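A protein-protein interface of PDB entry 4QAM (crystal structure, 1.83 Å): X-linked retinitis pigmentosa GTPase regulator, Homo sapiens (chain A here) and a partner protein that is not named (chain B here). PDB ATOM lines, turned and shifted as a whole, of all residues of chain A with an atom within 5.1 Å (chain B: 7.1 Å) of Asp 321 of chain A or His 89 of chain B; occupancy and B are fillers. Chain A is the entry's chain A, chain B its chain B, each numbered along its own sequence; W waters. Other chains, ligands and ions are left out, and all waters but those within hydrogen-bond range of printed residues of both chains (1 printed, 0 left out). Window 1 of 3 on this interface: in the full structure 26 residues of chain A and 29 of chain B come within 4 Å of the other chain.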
ATOM      1  N   PHE A 271     -12.579 -15.187  -7.611  1.00  0.00           N
ATOM      2  CA  PHE A 271     -12.519 -15.939  -6.354  1.00  0.00           C
ATOM      3  C   PHE A 271     -12.942 -15.085  -5.153  1.00  0.00           C
ATOM      4  O   PHE A 271     -12.863 -15.558  -4.026  1.00  0.00           O
ATOM      5  CB  PHE A 271     -11.090 -16.448  -6.113  1.00  0.00           C
ATOM      6  CG  PHE A 271     -10.468 -17.083  -7.352  1.00  0.00           C
ATOM      7  CD1 PHE A 271     -11.078 -18.195  -7.944  1.00  0.00           C
ATOM      8  CD2 PHE A 271      -9.344 -16.513  -7.979  1.00  0.00           C
ATOM      9  CE1 PHE A 271     -10.571 -18.813  -9.123  1.00  0.00           C
ATOM     10  CE2 PHE A 271      -8.797 -17.151  -9.143  1.00  0.00           C
ATOM     11  CZ  PHE A 271      -9.413 -18.284  -9.706  1.00  0.00           C
ATOM     12  N   GLN A 273     -11.791 -11.744  -4.640  1.00  0.00           N
ATOM     13  CA  GLN A 273     -10.682 -10.939  -4.146  1.00  0.00           C
ATOM     14  C   GLN A 273     -10.979  -9.477  -4.348  1.00  0.00           C
ATOM     15  O   GLN A 273     -10.196  -8.655  -3.873  1.00  0.00           O
ATOM     16  CB  GLN A 273      -9.295 -11.375  -4.772  1.00  0.00           C
ATOM     17  CG  GLN A 273      -9.149 -11.217  -6.293  1.00  0.00           C
ATOM     18  CD  GLN A 273      -9.571 -12.470  -7.115  1.00  0.00           C
ATOM     19  OE1 GLN A 273     -10.639 -13.113  -6.854  1.00  0.00           O
ATOM     20  NE2 GLN A 273      -8.763 -12.803  -8.161  1.00  0.00           N
ATOM     21  N   ASN A 305      -4.330 -14.095  -5.508  1.00  0.00           N
ATOM     22  CA  ASN A 305      -5.811 -14.207  -5.709  1.00  0.00           C
ATOM     23  C   ASN A 305      -6.618 -13.959  -4.385  1.00  0.00           C
ATOM     24  O   ASN A 305      -7.718 -14.422  -4.240  1.00  0.00           O
ATOM     25  CB  ASN A 305      -6.065 -15.614  -6.216  1.00  0.00           C
ATOM     26  CG  ASN A 305      -5.740 -15.697  -7.716  1.00  0.00           C
ATOM     27  OD1 ASN A 305      -6.128 -14.812  -8.516  1.00  0.00           O
ATOM     28  ND2 ASN A 305      -5.020 -16.646  -8.064  1.00  0.00           N
ATOM     29  N   HIS A 306      -5.998 -13.223  -3.461  1.00  0.00           N
ATOM     30  CA  HIS A 306      -6.730 -12.852  -2.245  1.00  0.00           C
ATOM     31  C   HIS A 306      -6.203 -11.543  -1.722  1.00  0.00           C
ATOM     32  O   HIS A 306      -5.187 -10.978  -2.258  1.00  0.00           O
ATOM     33  CB  HIS A 306      -6.731 -13.950  -1.212  1.00  0.00           C
ATOM     34  CG  HIS A 306      -5.469 -14.135  -0.434  1.00  0.00           C
ATOM     35  ND1 HIS A 306      -4.340 -14.763  -0.947  1.00  0.00           N
ATOM     36  CD2 HIS A 306      -5.201 -13.824   0.908  1.00  0.00           C
ATOM     37  CE1 HIS A 306      -3.389 -14.825   0.039  1.00  0.00           C
ATOM     38  NE2 HIS A 306      -3.955 -14.306   1.202  1.00  0.00           N
ATOM     39  N   PHE A 319     -10.366 -11.709   2.085  1.00  0.00           N
ATOM     40  CA  PHE A 319     -11.378 -12.084   1.101  1.00  0.00           C
ATOM     41  C   PHE A 319     -10.667 -12.552  -0.190  1.00  0.00           C
ATOM     42  O   PHE A 319      -9.479 -12.184  -0.426  1.00  0.00           O
ATOM     43  CB  PHE A 319     -12.382 -10.938   0.779  1.00  0.00           C
ATOM     44  CG  PHE A 319     -11.748  -9.568   0.519  1.00  0.00           C
ATOM     45  CD1 PHE A 319     -11.355  -8.757   1.596  1.00  0.00           C
ATOM     46  CD2 PHE A 319     -11.696  -9.020  -0.789  1.00  0.00           C
ATOM     47  CE1 PHE A 319     -10.841  -7.461   1.427  1.00  0.00           C
ATOM     48  CE2 PHE A 319     -11.181  -7.735  -0.958  1.00  0.00           C
ATOM     49  CZ  PHE A 319     -10.760  -6.953   0.154  1.00  0.00           C
ATOM     50  N   GLY A 320     -11.336 -13.436  -0.917  1.00  0.00           N
ATOM     51  CA  GLY A 320     -10.750 -13.980  -2.144  1.00  0.00           C
ATOM     52  C   GLY A 320     -10.605 -15.474  -2.024  1.00  0.00           C
ATOM     53  O   GLY A 320     -11.404 -16.175  -1.309  1.00  0.00           O
ATOM     54  N   ASP A 321      -9.610 -15.998  -2.746  1.00  0.00           N
ATOM     55  CA  ASP A 321      -9.462 -17.445  -2.928  1.00  0.00           C
ATOM     56  C   ASP A 321      -9.090 -18.109  -1.595  1.00  0.00           C
ATOM     57  O   ASP A 321      -8.133 -17.646  -0.958  1.00  0.00           O
ATOM     58  CB  ASP A 321      -8.321 -17.651  -3.975  1.00  0.00           C
ATOM     59  CG  ASP A 321      -7.947 -19.128  -4.244  1.00  0.00           C
ATOM     60  OD1 ASP A 321      -8.646 -20.088  -3.858  1.00  0.00           O
ATOM     61  OD2 ASP A 321      -6.858 -19.307  -4.924  1.00  0.00           O
ATOM     62  N   GLY A 322      -9.858 -19.122  -1.171  1.00  0.00           N
ATOM     63  CA  GLY A 322      -9.729 -19.723   0.188  1.00  0.00           C
ATOM     64  C   GLY A 322      -8.810 -20.988   0.099  1.00  0.00           C
ATOM     65  O   GLY A 322      -8.541 -21.648   1.138  1.00  0.00           O
ATOM     66  N   ARG A 323      -8.312 -21.345  -1.097  1.00  0.00           N
ATOM     67  CA  ARG A 323      -7.539 -22.664  -1.162  1.00  0.00           C
ATOM     68  C   ARG A 323      -6.374 -22.716  -0.196  1.00  0.00           C
ATOM     69  O   ARG A 323      -5.728 -21.661   0.061  1.00  0.00           O
ATOM     70  CB  ARG A 323      -6.945 -22.892  -2.572  1.00  0.00           C
ATOM     71  CG  ARG A 323      -8.069 -23.387  -3.473  1.00  0.00           C
ATOM     72  CD  ARG A 323      -7.624 -23.377  -4.915  1.00  0.00           C
ATOM     73  NE  ARG A 323      -8.431 -24.454  -5.566  1.00  0.00           N
ATOM     74  CZ  ARG A 323      -8.382 -24.605  -6.870  1.00  0.00           C
ATOM     75  NH1 ARG A 323      -7.592 -23.754  -7.557  1.00  0.00           N
ATOM     76  NH2 ARG A 323      -9.038 -25.592  -7.466  1.00  0.00           N
ATOM     77  N   LYS A 326      -5.375 -20.146   2.957  1.00  0.00           N
ATOM     78  CA  LYS A 326      -4.551 -18.947   2.864  1.00  0.00           C
ATOM     79  C   LYS A 326      -5.272 -17.651   3.256  1.00  0.00           C
ATOM     80  O   LYS A 326      -4.638 -16.623   3.424  1.00  0.00           O
ATOM     81  CB  LYS A 326      -3.896 -18.792   1.447  1.00  0.00           C
ATOM     82  CG  LYS A 326      -4.903 -18.337   0.349  1.00  0.00           C
ATOM     83  CD  LYS A 326      -4.190 -18.555  -1.040  1.00  0.00           C
ATOM     84  CE  LYS A 326      -5.279 -18.443  -2.138  1.00  0.00           C
ATOM     85  NZ  LYS A 326      -4.587 -18.410  -3.476  1.00  0.00           N
ATOM     86  N   LEU A 327      -6.578 -17.707   3.395  1.00  0.00           N
ATOM     87  CA  LEU A 327      -7.296 -16.565   3.973  1.00  0.00           C
ATOM     88  C   LEU A 327      -6.993 -16.310   5.444  1.00  0.00           C
ATOM     89  O   LEU A 327      -7.411 -15.285   5.976  1.00  0.00           O
ATOM     90  CB  LEU A 327      -8.825 -16.699   3.757  1.00  0.00           C
ATOM     91  CG  LEU A 327      -9.184 -16.577   2.223  1.00  0.00           C
ATOM     92  CD1 LEU A 327     -10.686 -16.843   2.135  1.00  0.00           C
ATOM     93  CD2 LEU A 327      -8.769 -15.222   1.531  1.00  0.00           C
ATOM     94  N   PHE A 334     -12.145 -24.954   3.734  1.00  0.00           N
ATOM     95  CA  PHE A 334     -11.838 -23.742   3.063  1.00  0.00           C
ATOM     96  C   PHE A 334     -12.910 -23.421   2.013  1.00  0.00           C
ATOM     97  O   PHE A 334     -13.594 -24.334   1.489  1.00  0.00           O
ATOM     98  CB  PHE A 334     -10.538 -23.982   2.287  1.00  0.00           C
ATOM     99  CG  PHE A 334      -9.429 -24.598   3.120  1.00  0.00           C
ATOM    100  CD1 PHE A 334      -8.647 -25.595   2.583  1.00  0.00           C
ATOM    101  CD2 PHE A 334      -9.172 -24.099   4.413  1.00  0.00           C
ATOM    102  CE1 PHE A 334      -7.587 -26.135   3.377  1.00  0.00           C
ATOM    103  CE2 PHE A 334      -8.114 -24.632   5.201  1.00  0.00           C
ATOM    104  CZ  PHE A 334      -7.325 -25.636   4.649  1.00  0.00           C
ATOM    105  N   THR A 335     -13.012 -22.150   1.664  1.00  0.00           N
ATOM    106  CA  THR A 335     -14.023 -21.694   0.725  1.00  0.00           C
ATOM    107  C   THR A 335     -13.584 -20.347   0.233  1.00  0.00           C
ATOM    108  O   THR A 335     -12.960 -19.623   0.979  1.00  0.00           O
ATOM    109  CB  THR A 335     -15.472 -21.626   1.348  1.00  0.00           C
ATOM    110  OG1 THR A 335     -16.372 -21.069   0.383  1.00  0.00           O
ATOM    111  CG2 THR A 335     -15.490 -20.755   2.518  1.00  0.00           C
ATOM    112  N   ASN A 336     -13.901 -20.014  -1.008  1.00  0.00           N
ATOM    113  CA  ASN A 336     -13.735 -18.595  -1.450  1.00  0.00           C
ATOM    114  C   ASN A 336     -14.656 -17.696  -0.595  1.00  0.00           C
ATOM    115  O   ASN A 336     -15.755 -18.129  -0.207  1.00  0.00           O
ATOM    116  CB  ASN A 336     -14.099 -18.411  -2.899  1.00  0.00           C
ATOM    117  CG  ASN A 336     -13.059 -19.107  -3.807  1.00  0.00           C
ATOM    118  OD1 ASN A 336     -11.974 -19.414  -3.308  1.00  0.00           O
ATOM    119  ND2 ASN A 336     -13.391 -19.366  -5.061  1.00  0.00           N
ATOM    120  N   GLU B  36     -13.181 -31.325  -3.087  1.00  0.00           N
ATOM    121  CA  GLU B  36     -13.372 -29.890  -3.428  1.00  0.00           C
ATOM    122  C   GLU B  36     -14.356 -29.672  -4.523  1.00  0.00           C
ATOM    123  O   GLU B  36     -14.176 -30.239  -5.605  1.00  0.00           O
ATOM    124  CB  GLU B  36     -12.019 -29.244  -3.823  1.00  0.00           C
ATOM    125  CG  GLU B  36     -12.176 -27.690  -4.031  1.00  0.00           C
ATOM    126  CD  GLU B  36     -10.860 -26.991  -4.457  1.00  0.00           C
ATOM    127  OE1 GLU B  36     -10.000 -27.672  -4.961  1.00  0.00           O
ATOM    128  OE2 GLU B  36     -10.647 -25.772  -4.344  1.00  0.00           O
ATOM    129  N   ILE B  37     -15.329 -28.771  -4.310  1.00  0.00           N
ATOM    130  CA  ILE B  37     -16.238 -28.360  -5.367  1.00  0.00           C
ATOM    131  C   ILE B  37     -15.560 -27.088  -5.960  1.00  0.00           C
ATOM    132  O   ILE B  37     -15.350 -26.099  -5.231  1.00  0.00           O
ATOM    133  CB  ILE B  37     -17.581 -28.033  -4.752  1.00  0.00           C
ATOM    134  CG1 ILE B  37     -18.206 -29.353  -4.260  1.00  0.00           C
ATOM    135  CG2 ILE B  37     -18.446 -27.417  -5.844  1.00  0.00           C
ATOM    136  CD1 ILE B  37     -19.618 -29.116  -3.656  1.00  0.00           C
ATOM    137  N   VAL B  38     -15.035 -27.194  -7.177  1.00  0.00           N
ATOM    138  CA  VAL B  38     -14.192 -26.095  -7.693  1.00  0.00           C
ATOM    139  C   VAL B  38     -15.006 -25.047  -8.360  1.00  0.00           C
ATOM    140  O   VAL B  38     -15.019 -23.850  -7.878  1.00  0.00           O
ATOM    141  CB  VAL B  38     -13.191 -26.651  -8.755  1.00  0.00           C
ATOM    142  CG1 VAL B  38     -12.264 -25.533  -9.282  1.00  0.00           C
ATOM    143  CG2 VAL B  38     -12.275 -27.720  -8.098  1.00  0.00           C
ATOM    144  N   SER B  39     -15.695 -25.380  -9.458  1.00  0.00           N
ATOM    145  CA  SER B  39     -16.317 -24.283 -10.173  1.00  0.00           C
ATOM    146  C   SER B  39     -17.380 -24.842 -11.135  1.00  0.00           C
ATOM    147  O   SER B  39     -17.427 -26.055 -11.324  1.00  0.00           O
ATOM    148  CB  SER B  39     -15.224 -23.533 -11.019  1.00  0.00           C
ATOM    149  OG  SER B  39     -14.587 -24.359 -12.012  1.00  0.00           O
ATOM    150  N   THR B  73     -21.803 -25.855  -0.573  1.00  0.00           N
ATOM    151  CA  THR B  73     -20.842 -24.727  -0.692  1.00  0.00           C
ATOM    152  C   THR B  73     -21.408 -23.631   0.247  1.00  0.00           C
ATOM    153  O   THR B  73     -22.581 -23.412   0.282  1.00  0.00           O
ATOM    154  CB  THR B  73     -20.715 -24.212  -2.133  1.00  0.00           C
ATOM    155  OG1 THR B  73     -22.030 -23.844  -2.592  1.00  0.00           O
ATOM    156  CG2 THR B  73     -20.212 -25.272  -3.084  1.00  0.00           C
ATOM    157  N   PRO B  74     -20.552 -22.971   1.042  1.00  0.00           N
ATOM    158  CA  PRO B  74     -21.128 -22.107   2.076  1.00  0.00           C
ATOM    159  C   PRO B  74     -21.642 -20.825   1.450  1.00  0.00           C
ATOM    160  O   PRO B  74     -22.233 -20.036   2.119  1.00  0.00           O
ATOM    161  CB  PRO B  74     -19.860 -21.700   2.886  1.00  0.00           C
ATOM    162  CG  PRO B  74     -18.900 -22.842   2.756  1.00  0.00           C
ATOM    163  CD  PRO B  74     -19.179 -23.464   1.380  1.00  0.00           C
ATOM    164  N   LEU B  77     -23.616 -18.251  -5.557  1.00  0.00           N
ATOM    165  CA  LEU B  77     -23.002 -17.297  -6.457  1.00  0.00           C
ATOM    166  C   LEU B  77     -23.983 -16.979  -7.611  1.00  0.00           C
ATOM    167  O   LEU B  77     -24.714 -17.863  -8.077  1.00  0.00           O
ATOM    168  CB  LEU B  77     -21.707 -17.948  -7.091  1.00  0.00           C
ATOM    169  CG  LEU B  77     -20.564 -18.083  -6.041  1.00  0.00           C
ATOM    170  CD1 LEU B  77     -19.275 -18.814  -6.651  1.00  0.00           C
ATOM    171  CD2 LEU B  77     -20.267 -16.736  -5.289  1.00  0.00           C
ATOM    172  N   ILE B  86     -18.239 -19.739 -12.488  1.00  0.00           N
ATOM    173  CA  ILE B  86     -18.225 -19.304 -11.125  1.00  0.00           C
ATOM    174  C   ILE B  86     -17.400 -20.273 -10.286  1.00  0.00           C
ATOM    175  O   ILE B  86     -17.406 -21.452 -10.510  1.00  0.00           O
ATOM    176  CB  ILE B  86     -19.673 -19.160 -10.578  1.00  0.00           C
ATOM    177  CG1 ILE B  86     -20.654 -20.318 -11.004  1.00  0.00           C
ATOM    178  CG2 ILE B  86     -20.247 -17.883 -11.245  1.00  0.00           C
ATOM    179  CD1 ILE B  86     -21.965 -20.269 -10.116  1.00  0.00           C
ATOM    180  N   HIS B  87     -16.755 -19.745  -9.258  1.00  0.00           N
ATOM    181  CA  HIS B  87     -15.698 -20.499  -8.557  1.00  0.00           C
ATOM    182  C   HIS B  87     -15.982 -20.522  -7.083  1.00  0.00           C
ATOM    183  O   HIS B  87     -16.009 -19.462  -6.389  1.00  0.00           O
ATOM    184  CB  HIS B  87     -14.329 -19.791  -8.803  1.00  0.00           C
ATOM    185  CG  HIS B  87     -14.003 -19.643 -10.253  1.00  0.00           C
ATOM    186  ND1 HIS B  87     -13.185 -20.473 -10.933  1.00  0.00           N
ATOM    187  CD2 HIS B  87     -14.457 -18.691 -11.179  1.00  0.00           C
ATOM    188  CE1 HIS B  87     -13.102 -20.079 -12.213  1.00  0.00           C
ATOM    189  NE2 HIS B  87     -13.855 -18.963 -12.353  1.00  0.00           N
ATOM    190  N   PHE B  88     -16.209 -21.735  -6.556  1.00  0.00           N
ATOM    191  CA  PHE B  88     -16.521 -21.909  -5.170  1.00  0.00           C
ATOM    192  C   PHE B  88     -15.299 -22.187  -4.348  1.00  0.00           C
ATOM    193  O   PHE B  88     -15.189 -21.635  -3.206  1.00  0.00           O
ATOM    194  CB  PHE B  88     -17.545 -23.058  -5.026  1.00  0.00           C
ATOM    195  CG  PHE B  88     -18.892 -22.739  -5.645  1.00  0.00           C
ATOM    196  CD1 PHE B  88     -19.872 -22.080  -4.908  1.00  0.00           C
ATOM    197  CD2 PHE B  88     -19.195 -23.172  -6.925  1.00  0.00           C
ATOM    198  CE1 PHE B  88     -21.184 -21.803  -5.495  1.00  0.00           C
ATOM    199  CE2 PHE B  88     -20.428 -22.886  -7.508  1.00  0.00           C
ATOM    200  CZ  PHE B  88     -21.440 -22.253  -6.741  1.00  0.00           C
ATOM    201  N   HIS B  89     -14.456 -23.108  -4.867  1.00  0.00           N
ATOM    202  CA  HIS B  89     -13.290 -23.637  -4.123  1.00  0.00           C
ATOM    203  C   HIS B  89     -13.659 -24.100  -2.738  1.00  0.00           C
ATOM    204  O   HIS B  89     -13.013 -23.744  -1.729  1.00  0.00           O
ATOM    205  CB  HIS B  89     -12.137 -22.581  -4.058  1.00  0.00           C
ATOM    206  CG  HIS B  89     -11.529 -22.233  -5.417  1.00  0.00           C
ATOM    207  ND1 HIS B  89     -10.457 -21.386  -5.537  1.00  0.00           N
ATOM    208  CD2 HIS B  89     -11.896 -22.591  -6.731  1.00  0.00           C
ATOM    209  CE1 HIS B  89     -10.139 -21.240  -6.825  1.00  0.00           C
ATOM    210  NE2 HIS B  89     -10.997 -22.000  -7.573  1.00  0.00           N
ATOM    211  N   PHE B  90     -14.727 -24.913  -2.634  1.00  0.00           N
ATOM    212  CA  PHE B  90     -15.177 -25.350  -1.312  1.00  0.00           C
ATOM    213  C   PHE B  90     -14.514 -26.701  -1.048  1.00  0.00           C
ATOM    214  O   PHE B  90     -14.818 -27.682  -1.780  1.00  0.00           O
ATOM    215  CB  PHE B  90     -16.699 -25.492  -1.308  1.00  0.00           C
ATOM    216  CG  PHE B  90     -17.235 -26.281  -0.141  1.00  0.00           C
ATOM    217  CD1 PHE B  90     -16.841 -25.954   1.141  1.00  0.00           C
ATOM    218  CD2 PHE B  90     -18.193 -27.330  -0.328  1.00  0.00           C
ATOM    219  CE1 PHE B  90     -17.362 -26.668   2.266  1.00  0.00           C
ATOM    220  CE2 PHE B  90     -18.676 -28.111   0.771  1.00  0.00           C
ATOM    221  CZ  PHE B  90     -18.245 -27.772   2.069  1.00  0.00           C
ATOM    222  N   SER B  91     -13.629 -26.777  -0.036  1.00  0.00           N
ATOM    223  CA  SER B  91     -12.909 -28.024   0.284  1.00  0.00           C
ATOM    224  C   SER B  91     -13.346 -28.579   1.636  1.00  0.00           C
ATOM    225  O   SER B  91     -13.500 -27.782   2.614  1.00  0.00           O
ATOM    226  CB  SER B  91     -11.398 -27.742   0.363  1.00  0.00           C
ATOM    227  OG  SER B  91     -10.763 -28.935   0.649  1.00  0.00           O
ATOM    228  N   LYS B  92     -13.480 -29.912   1.711  1.00  0.00           N
ATOM    229  CA  LYS B  92     -14.001 -30.610   2.920  1.00  0.00           C
ATOM    230  C   LYS B  92     -13.138 -31.877   3.108  1.00  0.00           C
ATOM    231  O   LYS B  92     -12.986 -32.662   2.159  1.00  0.00           O
ATOM    232  CB  LYS B  92     -15.482 -30.914   2.731  1.00  0.00           C
ATOM    233  CG  LYS B  92     -16.246 -31.759   3.772  1.00  0.00           C
ATOM    234  CD  LYS B  92     -16.577 -31.041   5.043  1.00  0.00           C
ATOM    235  CE  LYS B  92     -17.109 -32.106   5.960  1.00  0.00           C
ATOM    236  NZ  LYS B  92     -17.240 -31.493   7.308  1.00  0.00           N
ATOM    237  N   GLU B 160      -9.457 -30.881 -10.840  1.00  0.00           N
ATOM    238  CA  GLU B 160     -10.450 -30.213 -11.703  1.00  0.00           C
ATOM    239  C   GLU B 160     -10.981 -31.158 -12.799  1.00  0.00           C
ATOM    240  O   GLU B 160     -11.114 -30.738 -13.994  1.00  0.00           O
ATOM    241  CB  GLU B 160      -9.883 -28.908 -12.259  1.00  0.00           C
ATOM    242  CG  GLU B 160      -9.152 -28.187 -11.123  1.00  0.00           C
ATOM    243  CD  GLU B 160      -9.004 -26.698 -11.344  1.00  0.00           C
ATOM    244  OE1 GLU B 160      -9.513 -26.184 -12.386  1.00  0.00           O
ATOM    245  OE2 GLU B 160      -8.406 -26.046 -10.444  1.00  0.00           O
HETATM  246  O   HOH W   1     -17.646 -22.123  -1.644  1.00  0.00           O
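OD1 of Asp 321 of chain A is in hydrogen-bond range of ND1 of His 89 of chain B, at 2.8 Å. The side-chain carboxylate of Glu 36 of chain B is in salt-bridge range of the guanidinium group of Arg 323 of chain A (2.9 Å). The side-chain carboxylate (OE2) of Glu 160 of chain B is in salt-bridge range of the guanidinium group (NH2) of Arg 323 of chain A (3.1 Å). O of Phe 334 of chain A lies within hydrogen-bond range of N of Ser 91 of chain B, at 2.9 Å. The backbone carbonyl oxygen (O) of His 87 of chain B sits at hydrogen-bond distance from the side-chain amide nitrogen (ND2) of Asn 336 of chain A (2.9 Å). The backbone NH (N) of Asn 336 of chain A sits at hydrogen-bond distance from the backbone carbonyl oxygen (O) of Phe 88 of chain B (3.0 Å). ND1 of His 89 of chain B sits close to OD1 of Asn 336 of chain A, 3.3 Å away. O of Phe 334 of chain A sits close to O of His 89 of chain B (3.3 Å).
The backbone NH (N) of Phe 271 of chain A lies within hydrogen-bond range of the side-chain amide oxygen (OE1) of Gln 273 of chain A, 2.9 Å away. O of Asn 305 of chain A is in hydrogen-bond range of N of Asp 321 of chain A. OD1 of Asp 321 of chain A sits at hydrogen-bond distance from N of Arg 323 of chain A (3.1 Å). OD1 of Asp 321 of chain A sits close to OD1 of Asn 336 of chain A, at 3.4 Å. The backbone NH (N) of Gly 322 of chain A is in hydrogen-bond range of the side-chain amide oxygen (OD1) of Asn 336 of chain A (3.0 Å). The backbone NH of Ile 37 of chain B lies within hydrogen-bond range of the backbone carbonyl oxygen of Phe 90 of chain B, at 2.8 Å.
Among the printed residues, pairs that only touch across the chains: Thr 335 of chain A with His 89 of chain B (3.4 Å), Phe 271 of chain A with His 89 of chain B (3.4 Å), Phe 334 of chain A with Phe 90 of chain B (3.4 Å), Arg 323 of chain A with His 89 of chain B (3.5 Å), Phe 271 of chain A with His 87 of chain B (3.6 Å), Arg 323 of chain A with Val 38 of chain B (3.7 Å), Thr 335 of chain A with Phe 88 of chain B (3.8 Å) and Thr 335 of chain A with Pro 74 of chain B (3.8 Å).
Asn 305 of chain A touches none of the printed residues of chain B. Phe 319 of chain A touches none of the printed residues of chain B. Asp 321 of chain A touches one residue of chain B. Of the printed residues of chain B, Thr 335 of chain A touches Pro 74 (3.8 Å), Phe 88 (3.8 Å) and His 89 (3.4 Å). Of the printed residues of chain B, Asn 336 of chain A touches His 87, Phe 88 and His 89. Printed residues of chain A within 4 Å of Glu 36 of chain B: Arg 323 (2.9 Å). Printed residues of chain A within 4 Å of His 87 of chain B: Phe 271 (3.6 Å) and Asn 336 (2.9 Å). Printed residues of chain A within 4 Å of His 89 of chain B: Phe 271 (3.4 Å), Asp 321 (2.8 Å), Arg 323 (3.5 Å), Phe 334 (3.3 Å), Thr 335 (3.4 Å) and Asn 336 (3.3 Å). Of the printed residues of chain A, Ser 91 of chain B touches Phe 334. The nearest residue of chain A that does not touch His 89 of chain B is Gly 322 of chain A (5.0 Å). The nearest printed residue of chain A that does not touch Phe 88 of chain B is Phe 334 of chain A (5.6 Å).
Hydrophobic or aromatic side chains of chain A within 4 Å of the printed part of chain B: Phe 271. Hydrophobic or aromatic side chains of chain B that line the printed part of chain A: Val 38, Pro 74, His 87, His 89 and Phe 90.
Water W1 bridges OG1 of Thr 335 of chain A (2.6 Å) and O of Phe 88 of chain B (3.0 Å).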
